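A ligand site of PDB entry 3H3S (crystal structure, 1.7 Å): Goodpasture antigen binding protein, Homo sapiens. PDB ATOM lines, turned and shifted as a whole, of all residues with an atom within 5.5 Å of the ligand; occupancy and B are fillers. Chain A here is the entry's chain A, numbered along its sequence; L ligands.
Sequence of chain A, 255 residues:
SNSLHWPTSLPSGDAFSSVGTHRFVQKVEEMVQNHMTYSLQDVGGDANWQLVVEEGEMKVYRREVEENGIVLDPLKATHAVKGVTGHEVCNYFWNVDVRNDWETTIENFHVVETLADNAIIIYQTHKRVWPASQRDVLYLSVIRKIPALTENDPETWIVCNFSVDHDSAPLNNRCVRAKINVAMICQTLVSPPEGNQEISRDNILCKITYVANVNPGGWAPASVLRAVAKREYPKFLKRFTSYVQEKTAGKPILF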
ATOM      1  N   PHE A  93     -11.675  36.880  16.095  1.00  0.00           N
ATOM      2  CA  PHE A  93     -12.850  36.031  16.170  1.00  0.00           C
ATOM      3  C   PHE A  93     -12.639  34.898  15.166  1.00  0.00           C
ATOM      4  O   PHE A  93     -13.031  33.764  15.430  1.00  0.00           O
ATOM      5  CB  PHE A  93     -14.090  36.815  15.758  1.00  0.00           C
ATOM      6  CG  PHE A  93     -15.371  36.000  15.813  1.00  0.00           C
ATOM      7  CD1 PHE A  93     -15.766  35.428  17.029  1.00  0.00           C
ATOM      8  CD2 PHE A  93     -16.156  35.808  14.673  1.00  0.00           C
ATOM      9  CE1 PHE A  93     -16.934  34.684  17.128  1.00  0.00           C
ATOM     10  CE2 PHE A  93     -17.332  35.042  14.772  1.00  0.00           C
ATOM     11  CZ  PHE A  93     -17.703  34.484  16.022  1.00  0.00           C
ATOM     12  N   ARG A  99      -8.471  30.410  19.085  1.00  0.00           N
ATOM     13  CA  ARG A  99      -9.822  30.006  19.447  1.00  0.00           C
ATOM     14  C   ARG A  99      -9.924  29.542  20.908  1.00  0.00           C
ATOM     15  O   ARG A  99     -10.814  29.944  21.624  1.00  0.00           O
ATOM     16  CB  ARG A  99     -10.365  28.917  18.501  1.00  0.00           C
ATOM     17  CG  ARG A  99     -11.715  28.324  18.933  1.00  0.00           C
ATOM     18  CD  ARG A  99     -12.896  29.168  18.459  1.00  0.00           C
ATOM     19  NE  ARG A  99     -12.522  30.184  17.479  1.00  0.00           N
ATOM     20  CZ  ARG A  99     -12.741  30.112  16.171  1.00  0.00           C
ATOM     21  NH1 ARG A  99     -12.353  31.114  15.419  1.00  0.00           N
ATOM     22  NH2 ARG A  99     -13.342  29.078  15.608  1.00  0.00           N
ATOM     23  N   TRP A 102     -10.248  31.923  24.171  1.00  0.00           N
ATOM     24  CA  TRP A 102     -11.447  32.670  24.573  1.00  0.00           C
ATOM     25  C   TRP A 102     -12.750  31.858  24.554  1.00  0.00           C
ATOM     26  O   TRP A 102     -13.670  32.160  25.299  1.00  0.00           O
ATOM     27  CB  TRP A 102     -11.583  33.998  23.757  1.00  0.00           C
ATOM     28  CG  TRP A 102     -11.772  33.787  22.260  1.00  0.00           C
ATOM     29  CD1 TRP A 102     -10.815  33.856  21.287  1.00  0.00           C
ATOM     30  CD2 TRP A 102     -13.004  33.422  21.584  1.00  0.00           C
ATOM     31  NE1 TRP A 102     -11.381  33.606  20.034  1.00  0.00           N
ATOM     32  CE2 TRP A 102     -12.717  33.325  20.199  1.00  0.00           C
ATOM     33  CE3 TRP A 102     -14.324  33.199  22.026  1.00  0.00           C
ATOM     34  CZ2 TRP A 102     -13.699  32.986  19.246  1.00  0.00           C
ATOM     35  CZ3 TRP A 102     -15.316  32.843  21.059  1.00  0.00           C
ATOM     36  CH2 TRP A 102     -14.976  32.746  19.689  1.00  0.00           C
ATOM     37  N   GLU A 103     -12.840  30.846  23.683  1.00  0.00           N
ATOM     38  CA  GLU A 103     -14.054  30.056  23.516  1.00  0.00           C
ATOM     39  C   GLU A 103     -14.142  29.067  24.664  1.00  0.00           C
ATOM     40  O   GLU A 103     -13.146  28.427  24.989  1.00  0.00           O
ATOM     41  CB  GLU A 103     -13.970  29.326  22.154  1.00  0.00           C
ATOM     42  CG  GLU A 103     -15.058  28.303  21.863  1.00  0.00           C
ATOM     43  CD  GLU A 103     -16.465  28.853  21.806  1.00  0.00           C
ATOM     44  OE1 GLU A 103     -16.953  29.168  20.678  1.00  0.00           O
ATOM     45  OE2 GLU A 103     -17.123  28.934  22.868  1.00  0.00           O
ATOM     46  N   THR A 105     -17.235  26.999  25.055  1.00  0.00           N
ATOM     47  CA  THR A 105     -18.373  26.086  24.881  1.00  0.00           C
ATOM     48  C   THR A 105     -18.018  24.911  24.013  1.00  0.00           C
ATOM     49  O   THR A 105     -18.867  24.098  23.701  1.00  0.00           O
ATOM     50  CB  THR A 105     -19.623  26.774  24.291  1.00  0.00           C
ATOM     51  OG1 THR A 105     -19.401  27.094  22.900  1.00  0.00           O
ATOM     52  CG2 THR A 105     -19.985  28.014  25.071  1.00  0.00           C
ATOM     53  N   ILE A 106     -16.753  24.805  23.624  1.00  0.00           N
ATOM     54  CA  ILE A 106     -16.335  23.784  22.692  1.00  0.00           C
ATOM     55  C   ILE A 106     -15.644  22.641  23.434  1.00  0.00           C
ATOM     56  O   ILE A 106     -14.924  22.867  24.419  1.00  0.00           O
ATOM     57  CB  ILE A 106     -15.328  24.322  21.701  1.00  0.00           C
ATOM     58  CG1 ILE A 106     -16.041  25.102  20.602  1.00  0.00           C
ATOM     59  CG2 ILE A 106     -14.576  23.222  21.014  1.00  0.00           C
ATOM     60  CD1 ILE A 106     -15.036  25.948  19.788  1.00  0.00           C
ATOM     61  N   GLN A 124     -16.642  21.024  14.798  1.00  0.00           N
ATOM     62  CA  GLN A 124     -16.395  21.101  16.230  1.00  0.00           C
ATOM     63  C   GLN A 124     -17.523  20.478  16.989  1.00  0.00           C
ATOM     64  O   GLN A 124     -18.657  20.468  16.502  1.00  0.00           O
ATOM     65  CB  GLN A 124     -16.166  22.563  16.703  1.00  0.00           C
ATOM     66  CG  GLN A 124     -17.376  23.489  16.622  1.00  0.00           C
ATOM     67  CD  GLN A 124     -16.947  24.961  16.669  1.00  0.00           C
ATOM     68  OE1 GLN A 124     -15.876  25.320  16.176  1.00  0.00           O
ATOM     69  NE2 GLN A 124     -17.779  25.795  17.261  1.00  0.00           N
ATOM     70  N   HIS A 126     -19.520  20.615  20.732  1.00  0.00           N
ATOM     71  CA  HIS A 126     -19.775  21.520  21.826  1.00  0.00           C
ATOM     72  C   HIS A 126     -20.002  20.744  23.138  1.00  0.00           C
ATOM     73  O   HIS A 126     -20.496  19.595  23.120  1.00  0.00           O
ATOM     74  CB  HIS A 126     -20.978  22.425  21.504  1.00  0.00           C
ATOM     75  CG  HIS A 126     -20.593  23.532  20.565  1.00  0.00           C
ATOM     76  ND1 HIS A 126     -20.234  24.790  21.021  1.00  0.00           N
ATOM     77  CD2 HIS A 126     -20.427  23.546  19.229  1.00  0.00           C
ATOM     78  CE1 HIS A 126     -19.874  25.537  19.981  1.00  0.00           C
ATOM     79  NE2 HIS A 126     -19.982  24.808  18.890  1.00  0.00           N
ATOM     80  N   LYS A 127     -19.633  21.379  24.242  1.00  0.00           N
ATOM     81  CA  LYS A 127     -19.963  20.880  25.584  1.00  0.00           C
ATOM     82  C   LYS A 127     -21.460  20.763  25.687  1.00  0.00           C
ATOM     83  O   LYS A 127     -22.203  21.438  24.964  1.00  0.00           O
ATOM     84  CB  LYS A 127     -19.458  21.868  26.648  1.00  0.00           C
ATOM     85  CG  LYS A 127     -17.934  21.930  26.712  1.00  0.00           C
ATOM     86  CD  LYS A 127     -17.476  22.850  27.839  1.00  0.00           C
ATOM     87  CE  LYS A 127     -16.043  23.300  27.642  1.00  0.00           C
ATOM     88  NZ  LYS A 127     -15.189  22.134  27.277  1.00  0.00           N
ATOM     89  N   VAL A 129     -24.253  21.913  26.968  1.00  0.00           N
ATOM     90  CA  VAL A 129     -24.847  23.014  27.700  1.00  0.00           C
ATOM     91  C   VAL A 129     -26.380  22.926  27.776  1.00  0.00           C
ATOM     92  O   VAL A 129     -27.028  23.647  28.536  1.00  0.00           O
ATOM     93  CB  VAL A 129     -24.408  24.407  27.099  1.00  0.00           C
ATOM     94  CG1 VAL A 129     -22.879  24.550  27.089  1.00  0.00           C
ATOM     95  CG2 VAL A 129     -24.968  24.600  25.714  1.00  0.00           C
ATOM     96  N   TRP A 130     -26.966  22.049  26.960  1.00  0.00           N
ATOM     97  CA  TRP A 130     -28.417  21.881  26.937  1.00  0.00           C
ATOM     98  C   TRP A 130     -28.762  20.546  27.580  1.00  0.00           C
ATOM     99  O   TRP A 130     -27.944  19.597  27.537  1.00  0.00           O
ATOM    100  CB  TRP A 130     -28.919  21.843  25.512  1.00  0.00           C
ATOM    101  CG  TRP A 130     -28.798  23.144  24.781  1.00  0.00           C
ATOM    102  CD1 TRP A 130     -28.815  24.415  25.301  1.00  0.00           C
ATOM    103  CD2 TRP A 130     -28.692  23.292  23.360  1.00  0.00           C
ATOM    104  NE1 TRP A 130     -28.694  25.349  24.287  1.00  0.00           N
ATOM    105  CE2 TRP A 130     -28.630  24.684  23.086  1.00  0.00           C
ATOM    106  CE3 TRP A 130     -28.634  22.389  22.302  1.00  0.00           C
ATOM    107  CZ2 TRP A 130     -28.516  25.174  21.786  1.00  0.00           C
ATOM    108  CZ3 TRP A 130     -28.538  22.872  21.017  1.00  0.00           C
ATOM    109  CH2 TRP A 130     -28.462  24.253  20.766  1.00  0.00           C
ATOM    110  N   ARG A 135     -24.258  18.293  20.855  1.00  0.00           N
ATOM    111  CA  ARG A 135     -24.339  18.820  19.480  1.00  0.00           C
ATOM    112  C   ARG A 135     -22.975  18.940  18.823  1.00  0.00           C
ATOM    113  O   ARG A 135     -21.974  19.265  19.489  1.00  0.00           O
ATOM    114  CB  ARG A 135     -25.002  20.192  19.433  1.00  0.00           C
ATOM    115  CG  ARG A 135     -26.475  20.175  19.121  1.00  0.00           C
ATOM    116  CD  ARG A 135     -27.265  19.376  20.181  1.00  0.00           C
ATOM    117  NE  ARG A 135     -28.641  19.379  19.774  1.00  0.00           N
ATOM    118  CZ  ARG A 135     -29.596  18.596  20.269  1.00  0.00           C
ATOM    119  NH1 ARG A 135     -29.311  17.750  21.253  1.00  0.00           N
ATOM    120  NH2 ARG A 135     -30.828  18.705  19.783  1.00  0.00           N
ATOM    121  N   ASP A 136     -22.922  18.703  17.509  1.00  0.00           N
ATOM    122  CA  ASP A 136     -21.745  19.123  16.733  1.00  0.00           C
ATOM    123  C   ASP A 136     -22.153  20.064  15.633  1.00  0.00           C
ATOM    124  O   ASP A 136     -23.330  20.302  15.436  1.00  0.00           O
ATOM    125  CB  ASP A 136     -20.898  17.952  16.178  1.00  0.00           C
ATOM    126  CG  ASP A 136     -21.683  17.042  15.239  1.00  0.00           C
ATOM    127  OD1 ASP A 136     -22.868  17.282  14.989  1.00  0.00           O
ATOM    128  OD2 ASP A 136     -21.067  16.059  14.772  1.00  0.00           O
ATOM    129  N   VAL A 137     -21.174  20.619  14.940  1.00  0.00           N
ATOM    130  CA  VAL A 137     -21.488  21.607  13.885  1.00  0.00           C
ATOM    131  C   VAL A 137     -20.348  21.605  12.894  1.00  0.00           C
ATOM    132  O   VAL A 137     -19.208  21.269  13.217  1.00  0.00           O
ATOM    133  CB  VAL A 137     -21.786  23.047  14.487  1.00  0.00           C
ATOM    134  CG1 VAL A 137     -20.614  23.544  15.282  1.00  0.00           C
ATOM    135  CG2 VAL A 137     -22.208  24.050  13.387  1.00  0.00           C
ATOM    136  N   TYR A 139     -19.080  24.053   9.749  1.00  0.00           N
ATOM    137  CA  TYR A 139     -19.364  25.383   9.166  1.00  0.00           C
ATOM    138  C   TYR A 139     -18.195  25.990   8.408  1.00  0.00           C
ATOM    139  O   TYR A 139     -17.013  25.757   8.710  1.00  0.00           O
ATOM    140  CB  TYR A 139     -19.812  26.395  10.234  1.00  0.00           C
ATOM    141  CG  TYR A 139     -18.771  26.650  11.350  1.00  0.00           C
ATOM    142  CD1 TYR A 139     -17.995  27.794  11.356  1.00  0.00           C
ATOM    143  CD2 TYR A 139     -18.640  25.759  12.435  1.00  0.00           C
ATOM    144  CE1 TYR A 139     -17.079  28.045  12.382  1.00  0.00           C
ATOM    145  CE2 TYR A 139     -17.715  25.994  13.444  1.00  0.00           C
ATOM    146  CZ  TYR A 139     -16.935  27.138  13.418  1.00  0.00           C
ATOM    147  OH  TYR A 139     -16.020  27.395  14.431  1.00  0.00           O
ATOM    148  N   ASN A 161     -20.003  32.695   9.889  1.00  0.00           N
ATOM    149  CA  ASN A 161     -19.879  31.248  10.160  1.00  0.00           C
ATOM    150  C   ASN A 161     -21.220  30.638   9.760  1.00  0.00           C
ATOM    151  O   ASN A 161     -22.262  30.952  10.366  1.00  0.00           O
ATOM    152  CB  ASN A 161     -19.632  30.964  11.660  1.00  0.00           C
ATOM    153  CG  ASN A 161     -18.271  31.460  12.154  1.00  0.00           C
ATOM    154  OD1 ASN A 161     -18.088  31.715  13.357  1.00  0.00           O
ATOM    155  ND2 ASN A 161     -17.344  31.630  11.233  1.00  0.00           N
ATOM    156  N   ALA A 178     -26.180  20.357  14.670  1.00  0.00           N
ATOM    157  CA  ALA A 178     -26.858  21.634  14.693  1.00  0.00           C
ATOM    158  C   ALA A 178     -26.493  22.320  13.385  1.00  0.00           C
ATOM    159  O   ALA A 178     -25.513  21.979  12.753  1.00  0.00           O
ATOM    160  CB  ALA A 178     -26.372  22.472  15.911  1.00  0.00           C
ATOM    161  N   ILE A 180     -26.004  26.400  11.776  1.00  0.00           N
ATOM    162  CA  ILE A 180     -25.821  27.771  12.245  1.00  0.00           C
ATOM    163  C   ILE A 180     -25.733  28.738  11.094  1.00  0.00           C
ATOM    164  O   ILE A 180     -25.348  28.377   9.988  1.00  0.00           O
ATOM    165  CB  ILE A 180     -24.542  27.912  13.148  1.00  0.00           C
ATOM    166  CG1 ILE A 180     -23.251  27.768  12.373  1.00  0.00           C
ATOM    167  CG2 ILE A 180     -24.563  26.874  14.317  1.00  0.00           C
ATOM    168  CD1 ILE A 180     -22.016  28.087  13.248  1.00  0.00           C
ATOM    169  N   VAL A 182     -24.216  32.601  11.560  1.00  0.00           N
ATOM    170  CA  VAL A 182     -23.748  33.567  12.573  1.00  0.00           C
ATOM    171  C   VAL A 182     -22.914  34.613  11.835  1.00  0.00           C
ATOM    172  O   VAL A 182     -22.214  34.280  10.893  1.00  0.00           O
ATOM    173  CB  VAL A 182     -22.900  32.784  13.623  1.00  0.00           C
ATOM    174  CG1 VAL A 182     -22.028  33.719  14.543  1.00  0.00           C
ATOM    175  CG2 VAL A 182     -23.818  31.881  14.459  1.00  0.00           C
ATOM    176  N   TYR A 210     -23.465  41.312  16.486  1.00  0.00           N
ATOM    177  CA  TYR A 210     -23.219  39.877  16.426  1.00  0.00           C
ATOM    178  C   TYR A 210     -24.597  39.259  16.312  1.00  0.00           C
ATOM    179  O   TYR A 210     -25.510  39.569  17.108  1.00  0.00           O
ATOM    180  CB  TYR A 210     -22.499  39.403  17.690  1.00  0.00           C
ATOM    181  CG  TYR A 210     -22.392  37.907  17.831  1.00  0.00           C
ATOM    182  CD1 TYR A 210     -23.349  37.192  18.548  1.00  0.00           C
ATOM    183  CD2 TYR A 210     -21.344  37.207  17.249  1.00  0.00           C
ATOM    184  CE1 TYR A 210     -23.251  35.806  18.671  1.00  0.00           C
ATOM    185  CE2 TYR A 210     -21.245  35.825  17.381  1.00  0.00           C
ATOM    186  CZ  TYR A 210     -22.207  35.144  18.075  1.00  0.00           C
ATOM    187  OH  TYR A 210     -22.079  33.773  18.200  1.00  0.00           O
ATOM    188  N   ALA A 212     -26.694  35.504  15.729  1.00  0.00           N
ATOM    189  CA  ALA A 212     -26.555  34.057  15.698  1.00  0.00           C
ATOM    190  C   ALA A 212     -27.940  33.439  15.467  1.00  0.00           C
ATOM    191  O   ALA A 212     -28.858  33.709  16.213  1.00  0.00           O
ATOM    192  CB  ALA A 212     -25.926  33.511  17.000  1.00  0.00           C
ATOM    193  N   VAL A 214     -29.316  29.719  15.392  1.00  0.00           N
ATOM    194  CA  VAL A 214     -28.857  28.377  15.646  1.00  0.00           C
ATOM    195  C   VAL A 214     -30.097  27.468  15.602  1.00  0.00           C
ATOM    196  O   VAL A 214     -31.144  27.806  16.189  1.00  0.00           O
ATOM    197  CB  VAL A 214     -28.155  28.325  17.026  1.00  0.00           C
ATOM    198  CG1 VAL A 214     -27.809  26.936  17.452  1.00  0.00           C
ATOM    199  CG2 VAL A 214     -26.852  29.222  17.014  1.00  0.00           C
ATOM    200  N   VAL A 228     -30.129  29.250  28.783  1.00  0.00           N
ATOM    201  CA  VAL A 228     -28.747  28.981  28.439  1.00  0.00           C
ATOM    202  C   VAL A 228     -28.213  30.049  27.463  1.00  0.00           C
ATOM    203  O   VAL A 228     -27.093  30.516  27.621  1.00  0.00           O
ATOM    204  CB  VAL A 228     -28.550  27.589  27.790  1.00  0.00           C
ATOM    205  CG1 VAL A 228     -27.260  27.515  27.032  1.00  0.00           C
ATOM    206  CG2 VAL A 228     -28.589  26.462  28.865  1.00  0.00           C
ATOM    207  N   ALA A 229     -29.000  30.430  26.466  1.00  0.00           N
ATOM    208  CA  ALA A 229     -28.589  31.494  25.550  1.00  0.00           C
ATOM    209  C   ALA A 229     -28.396  32.843  26.284  1.00  0.00           C
ATOM    210  O   ALA A 229     -27.399  33.551  26.047  1.00  0.00           O
ATOM    211  CB  ALA A 229     -29.624  31.629  24.418  1.00  0.00           C
ATOM    212  N   GLU A 232     -24.999  32.417  28.212  1.00  0.00           N
ATOM    213  CA  GLU A 232     -23.813  32.072  27.471  1.00  0.00           C
ATOM    214  C   GLU A 232     -23.398  33.140  26.445  1.00  0.00           C
ATOM    215  O   GLU A 232     -22.230  33.372  26.287  1.00  0.00           O
ATOM    216  CB  GLU A 232     -23.968  30.723  26.786  1.00  0.00           C
ATOM    217  CG  GLU A 232     -23.887  29.545  27.768  1.00  0.00           C
ATOM    218  CD  GLU A 232     -22.580  29.521  28.589  1.00  0.00           C
ATOM    219  OE1 GLU A 232     -21.466  29.582  27.996  1.00  0.00           O
ATOM    220  OE2 GLU A 232     -22.671  29.402  29.846  1.00  0.00           O
ATOM    221  N   TYR A 233     -24.340  33.749  25.717  1.00  0.00           N
ATOM    222  CA  TYR A 233     -23.908  34.743  24.716  1.00  0.00           C
ATOM    223  C   TYR A 233     -23.265  35.971  25.363  1.00  0.00           C
ATOM    224  O   TYR A 233     -22.209  36.427  24.879  1.00  0.00           O
ATOM    225  CB  TYR A 233     -25.058  35.145  23.801  1.00  0.00           C
ATOM    226  CG  TYR A 233     -25.369  34.078  22.785  1.00  0.00           C
ATOM    227  CD1 TYR A 233     -24.600  33.958  21.637  1.00  0.00           C
ATOM    228  CD2 TYR A 233     -26.434  33.184  22.970  1.00  0.00           C
ATOM    229  CE1 TYR A 233     -24.866  32.997  20.694  1.00  0.00           C
ATOM    230  CE2 TYR A 233     -26.723  32.224  22.008  1.00  0.00           C
ATOM    231  CZ  TYR A 233     -25.931  32.128  20.892  1.00  0.00           C
ATOM    232  OH  TYR A 233     -26.150  31.198  19.931  1.00  0.00           O
ATOM    233  N   PHE A 236     -19.756  35.040  26.551  1.00  0.00           N
ATOM    234  CA  PHE A 236     -18.820  35.025  25.408  1.00  0.00           C
ATOM    235  C   PHE A 236     -18.482  36.427  24.956  1.00  0.00           C
ATOM    236  O   PHE A 236     -17.296  36.761  24.748  1.00  0.00           O
ATOM    237  CB  PHE A 236     -19.432  34.225  24.246  1.00  0.00           C
ATOM    238  CG  PHE A 236     -19.171  34.789  22.867  1.00  0.00           C
ATOM    239  CD1 PHE A 236     -17.907  34.794  22.309  1.00  0.00           C
ATOM    240  CD2 PHE A 236     -20.253  35.249  22.094  1.00  0.00           C
ATOM    241  CE1 PHE A 236     -17.707  35.295  20.983  1.00  0.00           C
ATOM    242  CE2 PHE A 236     -20.055  35.748  20.822  1.00  0.00           C
ATOM    243  CZ  PHE A 236     -18.782  35.775  20.265  1.00  0.00           C
HETATM  244  O1  LIG L   1     -19.734  32.420  17.780  1.00  0.00           O
HETATM  245  C1  LIG L   1     -19.252  31.627  18.612  1.00  0.00           C
HETATM  246  N1  LIG L   1     -18.441  30.600  18.352  1.00  0.00           N
HETATM  247  C2  LIG L   1     -17.811  30.342  17.037  1.00  0.00           C
HETATM  248  C3  LIG L   1     -16.383  29.802  17.238  1.00  0.00           C
HETATM  249  O2  LIG L   1     -16.444  28.543  17.979  1.00  0.00           O
HETATM  250  C4  LIG L   1     -18.609  29.340  16.176  1.00  0.00           C
HETATM  251  C5  LIG L   1     -19.968  29.990  16.205  1.00  0.00           C
HETATM  252  C6  LIG L   1     -21.086  29.394  16.974  1.00  0.00           C
HETATM  253  C7  LIG L   1     -21.111  28.081  17.461  1.00  0.00           C
HETATM  254  C8  LIG L   1     -22.200  27.714  18.238  1.00  0.00           C
HETATM  255  C9  LIG L   1     -23.223  28.597  18.578  1.00  0.00           C
HETATM  256  C10 LIG L   1     -23.197  29.904  18.104  1.00  0.00           C
HETATM  257  C11 LIG L   1     -22.105  30.265  17.339  1.00  0.00           C
HETATM  258  O3  LIG L   1     -20.167  31.046  15.272  1.00  0.00           O
HETATM  259  C12 LIG L   1     -19.515  31.864  20.082  1.00  0.00           C
HETATM  260  C13 LIG L   1     -20.910  31.471  20.489  1.00  0.00           C
HETATM  261  C14 LIG L   1     -21.005  31.405  22.017  1.00  0.00           C
HETATM  262  C15 LIG L   1     -22.441  31.144  22.477  1.00  0.00           C
HETATM  263  C16 LIG L   1     -22.790  29.662  22.617  1.00  0.00           C
HETATM  264  C17 LIG L   1     -24.228  29.458  23.089  1.00  0.00           C
HETATM  265  C18 LIG L   1     -24.497  27.975  23.294  1.00  0.00           C
HETATM  266  C19 LIG L   1     -25.377  27.411  22.185  1.00  0.00           C
HETATM  267  C20 LIG L   1     -25.409  25.885  22.194  1.00  0.00           C
HETATM  268  C21 LIG L   1     -24.129  25.183  21.744  1.00  0.00           C
HETATM  269  C22 LIG L   1     -24.495  23.961  20.910  1.00  0.00           C
HETATM  270  C23 LIG L   1     -25.052  24.358  19.556  1.00  0.00           C
HETATM  271  C24 LIG L   1     -24.115  23.901  18.458  1.00  0.00           C
HETATM  272  C25 LIG L   1     -24.105  24.915  17.343  1.00  0.00           C
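The side-chain carboxylate (OE1) of Glu 103 lies within hydrogen-bond range of an oxygen (O2) of the ligand (2.8 Å).
The side-chain amide nitrogen (NE2) of Gln 124 is in hydrogen-bond range of an oxygen (O2) of the ligand, at 3.1 Å.
The side-chain amide oxygen (OD1) of Asn 161 is in hydrogen-bond range of an oxygen (O3) of the ligand (2.9 Å).
The side-chain hydroxyl (OH) of Tyr 210 sits at hydrogen-bond distance from an oxygen (O1) of the ligand, 2.7 Å away.
The backbone NH (N) of His 126 lies within hydrogen-bond range of the backbone carbonyl oxygen (O) of Arg 135 (3.1 Å).
The backbone NH (N) of Thr 105 is in hydrogen-bond range of the side-chain carboxylate (OE2) of Glu 103, at 2.9 Å.
NE2 of Gln 124 is in hydrogen-bond range of NE2 of His 126 (2.9 Å).
The backbone NH of Val 182 sits at hydrogen-bond distance from the backbone carbonyl oxygen of Asn 161 (2.8 Å).
O of Gln 124 is in hydrogen-bond range of N of Val 137 (3.0 Å).
O of Phe 93 lies within hydrogen-bond range of NH1 of Arg 99.
NH2 of Arg 99 sits at hydrogen-bond distance from OH of Tyr 139.
The side-chain amide oxygen of Gln 124 lies within hydrogen-bond range of the side-chain hydroxyl of Tyr 139 (2.7 Å).
Residues that only touch the ligand: Phe 93 (3.4 Å), Arg 99 (3.5 Å), Ile 106 (3.5 Å), His 126 (3.6 Å), Val 129 (3.8 Å), Trp 130 (3.2 Å), Arg 135 (3.9 Å), Tyr 139 (3.7 Å), Ala 178 (3.6 Å), Ile 180 (3.6 Å), Val 182 (3.3 Å), Val 214 (3.9 Å), Glu 232 (3.9 Å), Tyr 233 (3.5 Å) and Phe 236 (3.9 Å).
Hydrophobic or aromatic side chains that line the ligand: Phe 93, Ile 106, His 126, Val 129, Trp 130, Tyr 139, Ala 178, Ile 180, Val 182, Tyr 210, Val 214, Tyr 233 and Phe 236.
Within 4 Å of the ligand: Phe 93, Arg 99, Glu 103, Ile 106, Gln 124, His 126, Val 129, Trp 130, Arg 135, Tyr 139, Asn 161, Ala 178, Ile 180, Val 182, Tyr 210, Val 214, Glu 232, Tyr 233 and Phe 236.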
